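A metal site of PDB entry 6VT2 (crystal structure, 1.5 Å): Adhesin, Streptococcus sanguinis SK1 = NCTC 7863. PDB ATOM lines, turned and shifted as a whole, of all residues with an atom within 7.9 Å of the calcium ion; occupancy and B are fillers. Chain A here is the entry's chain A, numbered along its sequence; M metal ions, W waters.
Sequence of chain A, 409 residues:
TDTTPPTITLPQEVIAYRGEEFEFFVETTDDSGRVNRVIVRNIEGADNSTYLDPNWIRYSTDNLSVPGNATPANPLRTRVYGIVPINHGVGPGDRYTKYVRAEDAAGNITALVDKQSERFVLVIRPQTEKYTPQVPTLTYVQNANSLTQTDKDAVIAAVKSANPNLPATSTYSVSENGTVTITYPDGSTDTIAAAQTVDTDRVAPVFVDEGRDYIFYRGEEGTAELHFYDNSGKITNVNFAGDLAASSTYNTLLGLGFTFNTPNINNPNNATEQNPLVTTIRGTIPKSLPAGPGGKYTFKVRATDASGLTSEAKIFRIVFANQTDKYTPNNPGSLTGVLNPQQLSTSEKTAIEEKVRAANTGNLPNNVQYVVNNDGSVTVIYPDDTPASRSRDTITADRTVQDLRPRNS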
ATOM      1  N   PRO A 126     -22.992 -24.387   4.389  1.00  0.00           N
ATOM      2  CA  PRO A 126     -21.622 -23.947   4.099  1.00  0.00           C
ATOM      3  C   PRO A 126     -21.612 -22.548   3.513  1.00  0.00           C
ATOM      4  O   PRO A 126     -22.563 -22.100   2.872  1.00  0.00           O
ATOM      5  CB  PRO A 126     -21.118 -24.996   3.097  1.00  0.00           C
ATOM      6  CG  PRO A 126     -22.395 -25.292   2.282  1.00  0.00           C
ATOM      7  CD  PRO A 126     -23.540 -25.306   3.388  1.00  0.00           C
ATOM      8  N   GLN A 127     -20.486 -21.867   3.700  1.00  0.00           N
ATOM      9  CA  GLN A 127     -20.372 -20.500   3.202  1.00  0.00           C
ATOM     10  C   GLN A 127     -20.556 -20.403   1.683  1.00  0.00           C
ATOM     11  O   GLN A 127     -21.098 -19.408   1.190  1.00  0.00           O
ATOM     12  CB  GLN A 127     -19.031 -19.900   3.581  1.00  0.00           C
ATOM     13  CG  GLN A 127     -19.016 -19.632   5.092  1.00  0.00           C
ATOM     14  CD  GLN A 127     -17.882 -18.795   5.573  1.00  0.00           C
ATOM     15  OE1 GLN A 127     -17.268 -18.113   4.790  1.00  0.00           O
ATOM     16  NE2 GLN A 127     -17.603 -18.847   6.873  1.00  0.00           N
ATOM     17  N   THR A 128     -20.188 -21.432   0.957  1.00  0.00           N
ATOM     18  CA  THR A 128     -20.324 -21.357  -0.482  1.00  0.00           C
ATOM     19  C   THR A 128     -21.769 -21.207  -0.926  1.00  0.00           C
ATOM     20  O   THR A 128     -22.002 -20.704  -2.028  1.00  0.00           O
ATOM     21  CB  THR A 128     -19.700 -22.552  -1.182  1.00  0.00           C
ATOM     22  OG1 THR A 128     -19.637 -22.223  -2.591  1.00  0.00           O
ATOM     23  CG2 THR A 128     -20.456 -23.806  -0.951  1.00  0.00           C
ATOM     24  N   GLU A 129     -22.741 -21.557  -0.081  1.00  0.00           N
ATOM     25  CA  GLU A 129     -24.117 -21.318  -0.487  1.00  0.00           C
ATOM     26  C   GLU A 129     -24.509 -19.854  -0.374  1.00  0.00           C
ATOM     27  O   GLU A 129     -25.488 -19.427  -0.992  1.00  0.00           O
ATOM     28  CB  GLU A 129     -25.042 -22.204   0.342  1.00  0.00           C
ATOM     29  CG  GLU A 129     -24.937 -23.631  -0.108  1.00  0.00           C
ATOM     30  CD  GLU A 129     -25.921 -24.524   0.590  1.00  0.00           C
ATOM     31  OE1 GLU A 129     -26.635 -24.042   1.505  1.00  0.00           O
ATOM     32  OE2 GLU A 129     -25.981 -25.695   0.222  1.00  0.00           O
ATOM     33  N   LYS A 130     -23.797 -19.092   0.428  1.00  0.00           N
ATOM     34  CA  LYS A 130     -24.047 -17.668   0.536  1.00  0.00           C
ATOM     35  C   LYS A 130     -23.401 -16.891  -0.603  1.00  0.00           C
ATOM     36  O   LYS A 130     -23.957 -15.902  -1.049  1.00  0.00           O
ATOM     37  CB  LYS A 130     -23.551 -17.214   1.912  1.00  0.00           C
ATOM     38  CG  LYS A 130     -23.599 -15.783   2.126  1.00  0.00           C
ATOM     39  CD  LYS A 130     -23.197 -15.478   3.574  1.00  0.00           C
ATOM     40  CE  LYS A 130     -23.399 -13.973   3.849  1.00  0.00           C
ATOM     41  NZ  LYS A 130     -22.593 -13.530   5.026  1.00  0.00           N
ATOM     42  N   TYR A 131     -22.255 -17.318  -1.099  1.00  0.00           N
ATOM     43  CA  TYR A 131     -21.447 -16.523  -2.023  1.00  0.00           C
ATOM     44  C   TYR A 131     -21.484 -17.137  -3.417  1.00  0.00           C
ATOM     45  O   TYR A 131     -21.342 -18.356  -3.596  1.00  0.00           O
ATOM     46  CB  TYR A 131     -20.024 -16.438  -1.482  1.00  0.00           C
ATOM     47  CG  TYR A 131     -19.951 -15.852  -0.111  1.00  0.00           C
ATOM     48  CD1 TYR A 131     -20.243 -14.499   0.099  1.00  0.00           C
ATOM     49  CD2 TYR A 131     -19.632 -16.630   0.982  1.00  0.00           C
ATOM     50  CE1 TYR A 131     -20.205 -13.949   1.387  1.00  0.00           C
ATOM     51  CE2 TYR A 131     -19.587 -16.086   2.267  1.00  0.00           C
ATOM     52  CZ  TYR A 131     -19.852 -14.722   2.444  1.00  0.00           C
ATOM     53  OH  TYR A 131     -19.831 -14.193   3.715  1.00  0.00           O
ATOM     54  N   THR A 132     -21.747 -16.285  -4.406  1.00  0.00           N
ATOM     55  CA  THR A 132     -21.757 -16.687  -5.803  1.00  0.00           C
ATOM     56  C   THR A 132     -20.742 -15.786  -6.521  1.00  0.00           C
ATOM     57  O   THR A 132     -21.028 -14.603  -6.760  1.00  0.00           O
ATOM     58  CB  THR A 132     -23.136 -16.568  -6.420  1.00  0.00           C
ATOM     59  OG1 THR A 132     -24.063 -17.387  -5.678  1.00  0.00           O
ATOM     60  CG2 THR A 132     -23.119 -17.061  -7.877  1.00  0.00           C
ATOM     61  N   PRO A 133     -19.575 -16.290  -6.871  1.00  0.00           N
ATOM     62  CA  PRO A 133     -18.537 -15.407  -7.441  1.00  0.00           C
ATOM     63  C   PRO A 133     -18.886 -14.981  -8.852  1.00  0.00           C
ATOM     64  O   PRO A 133     -19.505 -15.730  -9.620  1.00  0.00           O
ATOM     65  CB  PRO A 133     -17.264 -16.265  -7.443  1.00  0.00           C
ATOM     66  CG  PRO A 133     -17.593 -17.524  -6.674  1.00  0.00           C
ATOM     67  CD  PRO A 133     -19.122 -17.688  -6.763  1.00  0.00           C
ATOM     68  N   LEU A 166     -16.782 -11.018  -1.674  1.00  0.00           N
ATOM     69  CA  LEU A 166     -16.450 -12.330  -1.098  1.00  0.00           C
ATOM     70  C   LEU A 166     -15.728 -12.124   0.238  1.00  0.00           C
ATOM     71  O   LEU A 166     -15.189 -11.046   0.422  1.00  0.00           O
ATOM     72  CB  LEU A 166     -15.611 -13.149  -2.091  1.00  0.00           C
ATOM     73  CG  LEU A 166     -16.305 -13.597  -3.377  1.00  0.00           C
ATOM     74  CD1 LEU A 166     -15.367 -14.453  -4.216  1.00  0.00           C
ATOM     75  CD2 LEU A 166     -17.569 -14.385  -3.112  1.00  0.00           C
ATOM     76  N   TYR A 184     -13.586 -20.628   0.686  1.00  0.00           N
ATOM     77  CA  TYR A 184     -14.142 -19.754   1.713  1.00  0.00           C
ATOM     78  C   TYR A 184     -13.528 -20.186   3.010  1.00  0.00           C
ATOM     79  O   TYR A 184     -12.990 -21.194   3.246  1.00  0.00           O
ATOM     80  CB  TYR A 184     -15.650 -19.879   1.705  1.00  0.00           C
ATOM     81  CG  TYR A 184     -16.133 -19.370   0.406  1.00  0.00           C
ATOM     82  CD1 TYR A 184     -15.831 -18.096  -0.016  1.00  0.00           C
ATOM     83  CD2 TYR A 184     -16.783 -20.221  -0.419  1.00  0.00           C
ATOM     84  CE1 TYR A 184     -16.220 -17.682  -1.264  1.00  0.00           C
ATOM     85  CE2 TYR A 184     -17.225 -19.800  -1.631  1.00  0.00           C
ATOM     86  CZ  TYR A 184     -16.937 -18.533  -2.067  1.00  0.00           C
ATOM     87  OH  TYR A 184     -17.353 -18.130  -3.281  1.00  0.00           O
ATOM     88  N   SER A 188     -15.341 -24.508   2.413  1.00  0.00           N
ATOM     89  CA  SER A 188     -16.211 -24.763   1.262  1.00  0.00           C
ATOM     90  C   SER A 188     -15.630 -23.957   0.086  1.00  0.00           C
ATOM     91  O   SER A 188     -14.880 -23.060   0.272  1.00  0.00           O
ATOM     92  CB  SER A 188     -17.652 -24.462   1.545  1.00  0.00           C
ATOM     93  OG  SER A 188     -17.871 -23.116   1.730  1.00  0.00           O
ATOM     94  N   THR A 189     -15.979 -24.355  -1.121  1.00  0.00           N
ATOM     95  CA  THR A 189     -15.335 -23.755  -2.283  1.00  0.00           C
ATOM     96  C   THR A 189     -16.333 -23.354  -3.375  1.00  0.00           C
ATOM     97  O   THR A 189     -17.452 -23.772  -3.375  1.00  0.00           O
ATOM     98  CB  THR A 189     -14.327 -24.722  -2.905  1.00  0.00           C
ATOM     99  OG1 THR A 189     -15.030 -25.868  -3.384  1.00  0.00           O
ATOM    100  CG2 THR A 189     -13.248 -25.211  -1.959  1.00  0.00           C
ATOM    101  N   ASP A 190     -15.857 -22.509  -4.256  1.00  0.00           N
ATOM    102  CA  ASP A 190     -16.477 -22.260  -5.540  1.00  0.00           C
ATOM    103  C   ASP A 190     -15.381 -22.497  -6.574  1.00  0.00           C
ATOM    104  O   ASP A 190     -14.199 -22.332  -6.273  1.00  0.00           O
ATOM    105  CB  ASP A 190     -17.035 -20.884  -5.623  1.00  0.00           C
ATOM    106  CG  ASP A 190     -18.452 -20.810  -5.143  1.00  0.00           C
ATOM    107  OD1 ASP A 190     -19.255 -21.678  -5.526  1.00  0.00           O
ATOM    108  OD2 ASP A 190     -18.767 -19.861  -4.419  1.00  0.00           O
ATOM    109  N   THR A 191     -15.793 -22.869  -7.776  1.00  0.00           N
ATOM    110  CA  THR A 191     -14.873 -23.037  -8.901  1.00  0.00           C
ATOM    111  C   THR A 191     -15.274 -22.114 -10.036  1.00  0.00           C
ATOM    112  O   THR A 191     -16.469 -21.918 -10.337  1.00  0.00           O
ATOM    113  CB  THR A 191     -14.909 -24.476  -9.413  1.00  0.00           C
ATOM    114  OG1 THR A 191     -14.500 -25.405  -8.371  1.00  0.00           O
ATOM    115  CG2 THR A 191     -13.988 -24.634 -10.618  1.00  0.00           C
HETATM  116 CA    CA M   1     -21.118 -20.682  -4.121  1.00  0.00          CA
HETATM  117  O   HOH W   1     -22.166 -22.732  -4.535  1.00  0.00           O
HETATM  118  O   HOH W   2     -21.725 -20.232  -6.455  1.00  0.00           O
HETATM  119  O   HOH W   3     -23.432 -20.263  -4.262  1.00  0.00           O
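O of Thr 189 sits close to OG1 of Thr 128 (2.8 Å). The backbone NH (N) of Thr 128 is in hydrogen-bond range of the side-chain hydroxyl (OG) of Ser 188, at 3.0 Å. The side-chain hydroxyl (OH) of Tyr 131 lies within hydrogen-bond range of the side-chain amino group (NZ) of Lys 130, 3.1 Å away. The side-chain hydroxyl of Tyr 184 lies close to the side-chain carboxylate of Asp 190, 2.5 Å away.
The nearest printed residue that does not touch the calcium ion is Thr 132 (4.4 Å).
The calcium ion is bound by O of Thr 128 (2.3 Å), water W1 (2.3 Å), water W3 (2.4 Å), O of Tyr 131 (2.4 Å), water W2 (2.5 Å), OD2 of Asp 190 (2.5 Å), OD1 of Asp 190 (2.5 Å) and OG1 of Thr 128 (2.6 Å).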
